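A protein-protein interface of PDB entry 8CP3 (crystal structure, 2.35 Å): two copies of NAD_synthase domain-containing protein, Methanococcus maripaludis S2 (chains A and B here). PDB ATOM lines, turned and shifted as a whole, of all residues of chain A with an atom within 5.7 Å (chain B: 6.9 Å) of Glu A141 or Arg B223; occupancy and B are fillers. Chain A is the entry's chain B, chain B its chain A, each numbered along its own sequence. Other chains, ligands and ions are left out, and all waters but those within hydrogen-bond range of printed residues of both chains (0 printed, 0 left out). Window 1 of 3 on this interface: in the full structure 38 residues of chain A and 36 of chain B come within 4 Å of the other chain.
NH1 of Arg B221 is in salt-bridge range of OD2 of Asp A137, at 3.4 Å.
The side-chain carboxylate of Glu A141 is in salt-bridge range of the guanidinium group of Arg B223 (2.8 Å).
The side-chain hydroxyl (OH) of Tyr B219 sits at hydrogen-bond distance from the side-chain carboxylate (OE2) of Glu A141, at 3.3 Å.
The guanidinium group (NH1) of Arg B221 lies within salt-bridge range of the side-chain carboxylate (OE2) of Glu A141.
The guanidinium group of Arg B223 is in salt-bridge range of the side-chain carboxylate of Glu B232 (3.7 Å).
The guanidinium group (NH2) of Arg A143 lies within salt-bridge range of the side-chain carboxylate (OE1) of Glu A141, 2.5 Å away.
The backbone carbonyl oxygen (O) of Arg B223 is in hydrogen-bond range of the backbone NH (N) of Ile B230, 2.5 Å away.
NE of Arg B221 is in salt-bridge range of OE2 of Glu B207.
The backbone NH of Glu B232 is in hydrogen-bond range of the backbone carbonyl oxygen of Arg B221, at 2.7 Å.
OE1 of Glu B232 sits at hydrogen-bond distance from OH of Tyr B219 (2.5 Å).
Asp A137 touches Tyr B219 (O to CE1, 3.7 Å).
Phe A140 touches Tyr B219 (CD2 to CB, 3.7 Å).
Glu A141 touches three residues of chain B.
Arg B223 touches one residue of chain A.
Of the printed residues of chain A, Tyr B219 touches Asp A137, Phe A140 and Glu A141.
Of the printed residues of chain B, Phe A140 touches Tyr B219.
Of the printed residues of chain A, Arg B221 touches Asp A137 (3.2 Å) and Glu A141 (3.8 Å).
Printed residues of chain B within 4 Å of Asp A137: Tyr B219 and Arg B221.
The nearest residue of chain B that does not touch Glu A141 is Glu B232 (4.6 Å).
The nearest residue of chain A that does not touch Arg B223 is Arg A143 (4.7 Å).
Of the 7 printed residues of chain A, 3 touch a printed residue of chain B.
Hydrophobic or aromatic side chains of chain A within 4 Å of the printed part of chain B: Phe A140.
Of the 15 printed residues of chain B, 3 touch a printed residue of chain A.
Hydrophobic or aromatic side chains of chain B that line the printed part of chain A: Tyr B219.
Among the printed residues, 6 pairs touch across the chains.
No position is printed for both chains.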
ATOM      1  N   ASP A 137       2.019  28.249  24.395  1.00  0.00           N
ATOM      2  CA  ASP A 137       2.247  27.988  22.972  1.00  0.00           C
ATOM      3  C   ASP A 137       2.431  29.280  22.189  1.00  0.00           C
ATOM      4  O   ASP A 137       3.165  29.306  21.196  1.00  0.00           O
ATOM      5  CB  ASP A 137       1.081  27.190  22.372  1.00  0.00           C
ATOM      6  CG  ASP A 137       0.935  25.799  22.971  1.00  0.00           C
ATOM      7  OD1 ASP A 137       1.868  25.346  23.663  1.00  0.00           O
ATOM      8  OD2 ASP A 137      -0.120  25.160  22.753  1.00  0.00           O
ATOM      9  N   ASP A 138       1.743  30.355  22.600  1.00  0.00           N
ATOM     10  CA  ASP A 138       1.746  31.588  21.821  1.00  0.00           C
ATOM     11  C   ASP A 138       3.130  32.226  21.759  1.00  0.00           C
ATOM     12  O   ASP A 138       3.506  32.779  20.721  1.00  0.00           O
ATOM     13  CB  ASP A 138       0.751  32.593  22.397  1.00  0.00           C
ATOM     14  CG  ASP A 138      -0.698  32.138  22.267  1.00  0.00           C
ATOM     15  OD1 ASP A 138      -0.980  31.207  21.483  1.00  0.00           O
ATOM     16  OD2 ASP A 138      -1.556  32.756  22.922  1.00  0.00           O
ATOM     17  N   ILE A 139       3.920  32.132  22.832  1.00  0.00           N
ATOM     18  CA  ILE A 139       5.148  32.923  22.891  1.00  0.00           C
ATOM     19  C   ILE A 139       6.246  32.352  22.012  1.00  0.00           C
ATOM     20  O   ILE A 139       7.256  33.034  21.805  1.00  0.00           O
ATOM     21  CB  ILE A 139       5.641  33.094  24.341  1.00  0.00           C
ATOM     22  CG1 ILE A 139       6.306  31.824  24.842  1.00  0.00           C
ATOM     23  CG2 ILE A 139       4.459  33.488  25.270  1.00  0.00           C
ATOM     24  CD1 ILE A 139       6.772  31.924  26.275  1.00  0.00           C
ATOM     25  N   PHE A 140       6.071  31.133  21.472  1.00  0.00           N
ATOM     26  CA  PHE A 140       7.003  30.574  20.490  1.00  0.00           C
ATOM     27  C   PHE A 140       6.713  31.042  19.072  1.00  0.00           C
ATOM     28  O   PHE A 140       7.565  30.877  18.195  1.00  0.00           O
ATOM     29  CB  PHE A 140       6.970  29.037  20.474  1.00  0.00           C
ATOM     30  CG  PHE A 140       7.419  28.388  21.752  1.00  0.00           C
ATOM     31  CD1 PHE A 140       6.600  28.352  22.865  1.00  0.00           C
ATOM     32  CD2 PHE A 140       8.663  27.786  21.825  1.00  0.00           C
ATOM     33  CE1 PHE A 140       7.026  27.750  24.034  1.00  0.00           C
ATOM     34  CE2 PHE A 140       9.088  27.178  22.995  1.00  0.00           C
ATOM     35  CZ  PHE A 140       8.267  27.162  24.098  1.00  0.00           C
ATOM     36  N   GLU A 141       5.526  31.573  18.829  1.00  0.00           N
ATOM     37  CA  GLU A 141       5.084  32.068  17.538  1.00  0.00           C
ATOM     38  C   GLU A 141       5.405  33.549  17.395  1.00  0.00           C
ATOM     39  O   GLU A 141       5.862  34.204  18.335  1.00  0.00           O
ATOM     40  CB  GLU A 141       3.596  31.781  17.368  1.00  0.00           C
ATOM     41  CG  GLU A 141       3.318  30.299  17.615  1.00  0.00           C
ATOM     42  CD  GLU A 141       1.851  29.957  17.754  1.00  0.00           C
ATOM     43  OE1 GLU A 141       1.077  30.817  18.225  1.00  0.00           O
ATOM     44  OE2 GLU A 141       1.477  28.814  17.408  1.00  0.00           O
ATOM     45  N   ASP A 142       5.192  34.072  16.187  1.00  0.00           N
ATOM     46  CA  ASP A 142       5.482  35.476  15.916  1.00  0.00           C
ATOM     47  C   ASP A 142       4.223  36.275  16.210  1.00  0.00           C
ATOM     48  O   ASP A 142       3.384  36.512  15.339  1.00  0.00           O
ATOM     49  CB  ASP A 142       5.945  35.666  14.478  1.00  0.00           C
ATOM     50  CG  ASP A 142       6.272  37.114  14.170  1.00  0.00           C
ATOM     51  OD1 ASP A 142       6.798  37.799  15.077  1.00  0.00           O
ATOM     52  OD2 ASP A 142       6.006  37.566  13.033  1.00  0.00           O
ATOM     53  N   ARG A 143       4.089  36.707  17.459  1.00  0.00           N
ATOM     54  CA  ARG A 143       2.999  37.605  17.827  1.00  0.00           C
ATOM     55  C   ARG A 143       3.552  38.893  18.417  1.00  0.00           C
ATOM     56  O   ARG A 143       3.847  38.950  19.626  1.00  0.00           O
ATOM     57  CB  ARG A 143       2.041  36.919  18.798  1.00  0.00           C
ATOM     58  CG  ARG A 143       1.850  35.439  18.479  1.00  0.00           C
ATOM     59  CD  ARG A 143       0.679  34.801  19.227  1.00  0.00           C
ATOM     60  NE  ARG A 143       0.263  33.563  18.571  1.00  0.00           N
ATOM     61  CZ  ARG A 143      -0.967  33.063  18.583  1.00  0.00           C
ATOM     62  NH1 ARG A 143      -1.986  33.742  19.079  1.00  0.00           N
ATOM     63  NH2 ARG A 143      -1.181  31.856  18.070  1.00  0.00           N
ATOM     64  N   SER B 203      -6.885  17.688  15.762  1.00  0.00           N
ATOM     65  CA  SER B 203      -5.598  18.319  16.040  1.00  0.00           C
ATOM     66  C   SER B 203      -5.145  18.041  17.467  1.00  0.00           C
ATOM     67  O   SER B 203      -3.988  17.677  17.710  1.00  0.00           O
ATOM     68  CB  SER B 203      -5.688  19.823  15.793  1.00  0.00           C
ATOM     69  OG  SER B 203      -6.002  20.103  14.442  1.00  0.00           O
ATOM     70  N   GLU B 207      -1.630  16.273  18.829  1.00  0.00           N
ATOM     71  CA  GLU B 207      -0.658  16.837  19.761  1.00  0.00           C
ATOM     72  C   GLU B 207      -0.449  15.913  20.952  1.00  0.00           C
ATOM     73  O   GLU B 207       0.690  15.610  21.325  1.00  0.00           O
ATOM     74  CB  GLU B 207      -1.126  18.212  20.226  1.00  0.00           C
ATOM     75  CG  GLU B 207      -1.103  19.263  19.145  1.00  0.00           C
ATOM     76  CD  GLU B 207      -1.886  20.491  19.540  1.00  0.00           C
ATOM     77  OE1 GLU B 207      -2.051  20.703  20.760  1.00  0.00           O
ATOM     78  OE2 GLU B 207      -2.326  21.241  18.638  1.00  0.00           O
ATOM     79  N   TYR B 219       7.408  23.124  22.919  1.00  0.00           N
ATOM     80  CA  TYR B 219       6.291  23.453  22.037  1.00  0.00           C
ATOM     81  C   TYR B 219       6.069  22.382  20.975  1.00  0.00           C
ATOM     82  O   TYR B 219       7.003  21.986  20.271  1.00  0.00           O
ATOM     83  CB  TYR B 219       6.571  24.804  21.364  1.00  0.00           C
ATOM     84  CG  TYR B 219       5.700  25.140  20.166  1.00  0.00           C
ATOM     85  CD1 TYR B 219       4.566  25.934  20.313  1.00  0.00           C
ATOM     86  CD2 TYR B 219       6.026  24.694  18.885  1.00  0.00           C
ATOM     87  CE1 TYR B 219       3.777  26.262  19.230  1.00  0.00           C
ATOM     88  CE2 TYR B 219       5.226  25.009  17.793  1.00  0.00           C
ATOM     89  CZ  TYR B 219       4.107  25.798  17.976  1.00  0.00           C
ATOM     90  OH  TYR B 219       3.307  26.125  16.905  1.00  0.00           O
ATOM     91  N   ARG B 221       2.671  21.501  18.181  1.00  0.00           N
ATOM     92  CA  ARG B 221       1.329  21.768  17.679  1.00  0.00           C
ATOM     93  C   ARG B 221       1.117  21.047  16.359  1.00  0.00           C
ATOM     94  O   ARG B 221       2.064  20.802  15.607  1.00  0.00           O
ATOM     95  CB  ARG B 221       1.068  23.263  17.452  1.00  0.00           C
ATOM     96  CG  ARG B 221       1.307  24.133  18.662  1.00  0.00           C
ATOM     97  CD  ARG B 221       0.303  23.868  19.778  1.00  0.00           C
ATOM     98  NE  ARG B 221      -1.044  24.321  19.445  1.00  0.00           N
ATOM     99  CZ  ARG B 221      -1.430  25.591  19.428  1.00  0.00           C
ATOM    100  NH1 ARG B 221      -0.584  26.579  19.677  1.00  0.00           N
ATOM    101  NH2 ARG B 221      -2.696  25.880  19.144  1.00  0.00           N
ATOM    102  N   VAL B 222      -0.144  20.748  16.067  1.00  0.00           N
ATOM    103  CA  VAL B 222      -0.528  20.035  14.855  1.00  0.00           C
ATOM    104  C   VAL B 222      -1.554  20.891  14.124  1.00  0.00           C
ATOM    105  O   VAL B 222      -2.734  20.928  14.505  1.00  0.00           O
ATOM    106  CB  VAL B 222      -1.081  18.639  15.152  1.00  0.00           C
ATOM    107  CG1 VAL B 222      -1.500  17.981  13.854  1.00  0.00           C
ATOM    108  CG2 VAL B 222      -0.042  17.802  15.868  1.00  0.00           C
ATOM    109  N   ARG B 223      -1.111  21.578  13.072  1.00  0.00           N
ATOM    110  CA  ARG B 223      -1.995  22.390  12.247  1.00  0.00           C
ATOM    111  C   ARG B 223      -2.678  21.517  11.205  1.00  0.00           C
ATOM    112  O   ARG B 223      -2.111  20.531  10.721  1.00  0.00           O
ATOM    113  CB  ARG B 223      -1.222  23.507  11.545  1.00  0.00           C
ATOM    114  CG  ARG B 223      -0.478  24.460  12.465  1.00  0.00           C
ATOM    115  CD  ARG B 223      -1.434  25.193  13.386  1.00  0.00           C
ATOM    116  NE  ARG B 223      -0.755  26.177  14.224  1.00  0.00           N
ATOM    117  CZ  ARG B 223      -1.360  26.894  15.163  1.00  0.00           C
ATOM    118  NH1 ARG B 223      -2.653  26.752  15.417  1.00  0.00           N
ATOM    119  NH2 ARG B 223      -0.652  27.776  15.866  1.00  0.00           N
ATOM    120  N   TYR B 224      -3.904  21.896  10.852  1.00  0.00           N
ATOM    121  CA  TYR B 224      -4.730  21.144   9.914  1.00  0.00           C
ATOM    122  C   TYR B 224      -5.111  22.055   8.761  1.00  0.00           C
ATOM    123  O   TYR B 224      -5.695  23.121   8.980  1.00  0.00           O
ATOM    124  CB  TYR B 224      -5.985  20.596  10.596  1.00  0.00           C
ATOM    125  N   LEU B 225      -4.760  21.647   7.545  1.00  0.00           N
ATOM    126  CA  LEU B 225      -5.291  22.250   6.326  1.00  0.00           C
ATOM    127  C   LEU B 225      -5.786  21.132   5.422  1.00  0.00           C
ATOM    128  O   LEU B 225      -4.998  20.272   5.012  1.00  0.00           O
ATOM    129  CB  LEU B 225      -4.233  23.094   5.610  1.00  0.00           C
ATOM    130  N   ILE B 228      -4.998  17.582   6.343  1.00  0.00           N
ATOM    131  CA  ILE B 228      -3.575  17.256   6.352  1.00  0.00           C
ATOM    132  C   ILE B 228      -2.979  17.769   7.657  1.00  0.00           C
ATOM    133  O   ILE B 228      -3.208  18.924   8.039  1.00  0.00           O
ATOM    134  CB  ILE B 228      -2.844  17.857   5.138  1.00  0.00           C
ATOM    135  N   ALA B 229      -2.235  16.909   8.348  1.00  0.00           N
ATOM    136  CA  ALA B 229      -1.634  17.261   9.629  1.00  0.00           C
ATOM    137  C   ALA B 229      -0.299  17.975   9.407  1.00  0.00           C
ATOM    138  O   ALA B 229       0.635  17.389   8.850  1.00  0.00           O
ATOM    139  CB  ALA B 229      -1.457  16.004  10.477  1.00  0.00           C
ATOM    140  N   ILE B 230      -0.219  19.250   9.797  1.00  0.00           N
ATOM    141  CA  ILE B 230       1.035  20.006   9.798  1.00  0.00           C
ATOM    142  C   ILE B 230       1.576  20.033  11.223  1.00  0.00           C
ATOM    143  O   ILE B 230       0.991  20.668  12.108  1.00  0.00           O
ATOM    144  CB  ILE B 230       0.858  21.435   9.273  1.00  0.00           C
ATOM    145  CG1 ILE B 230       0.175  21.438   7.905  1.00  0.00           C
ATOM    146  CG2 ILE B 230       2.219  22.142   9.207  1.00  0.00           C
ATOM    147  CD1 ILE B 230      -0.155  22.827   7.401  1.00  0.00           C
ATOM    148  N   ILE B 231       2.706  19.372  11.451  1.00  0.00           N
ATOM    149  CA  ILE B 231       3.306  19.307  12.778  1.00  0.00           C
ATOM    150  C   ILE B 231       4.309  20.442  12.935  1.00  0.00           C
ATOM    151  O   ILE B 231       5.153  20.669  12.056  1.00  0.00           O
ATOM    152  CB  ILE B 231       3.979  17.948  12.997  1.00  0.00           C
ATOM    153  CG1 ILE B 231       3.079  16.835  12.465  1.00  0.00           C
ATOM    154  CG2 ILE B 231       4.291  17.759  14.459  1.00  0.00           C
ATOM    155  CD1 ILE B 231       3.739  15.480  12.453  1.00  0.00           C
ATOM    156  N   GLU B 232       4.222  21.154  14.059  1.00  0.00           N
ATOM    157  CA  GLU B 232       5.155  22.216  14.404  1.00  0.00           C
ATOM    158  C   GLU B 232       5.846  21.892  15.721  1.00  0.00           C
ATOM    159  O   GLU B 232       5.242  21.303  16.625  1.00  0.00           O
ATOM    160  CB  GLU B 232       4.433  23.551  14.519  1.00  0.00           C
ATOM    161  CG  GLU B 232       3.710  23.951  13.255  1.00  0.00           C
ATOM    162  CD  GLU B 232       3.162  25.352  13.346  1.00  0.00           C
ATOM    163  OE1 GLU B 232       3.414  26.008  14.385  1.00  0.00           O
ATOM    164  OE2 GLU B 232       2.456  25.785  12.404  1.00  0.00           O
ATOM    165  N   VAL B 263       2.549  15.522   7.637  1.00  0.00           N
ATOM    166  CA  VAL B 263       3.649  16.322   7.112  1.00  0.00           C
ATOM    167  C   VAL B 263       4.213  17.189   8.234  1.00  0.00           C
ATOM    168  O   VAL B 263       3.501  17.557   9.171  1.00  0.00           O
ATOM    169  CB  VAL B 263       3.182  17.183   5.910  1.00  0.00           C
ATOM    170  CG1 VAL B 263       4.329  17.867   5.308  1.00  0.00           C
ATOM    171  CG2 VAL B 263       2.527  16.337   4.817  1.00  0.00           C
ATOM    172  N   ASP B 265       6.299  20.674   9.216  1.00  0.00           N
ATOM    173  CA  ASP B 265       6.765  21.989   8.796  1.00  0.00           C
ATOM    174  C   ASP B 265       8.257  22.111   9.072  1.00  0.00           C
ATOM    175  O   ASP B 265       8.689  21.991  10.219  1.00  0.00           O
ATOM    176  CB  ASP B 265       5.979  23.071   9.533  1.00  0.00           C
ATOM    177  CG  ASP B 265       6.243  24.470   8.993  1.00  0.00           C
ATOM    178  OD1 ASP B 265       7.177  24.649   8.173  1.00  0.00           O
ATOM    179  OD2 ASP B 265       5.469  25.388   9.351  1.00  0.00           O
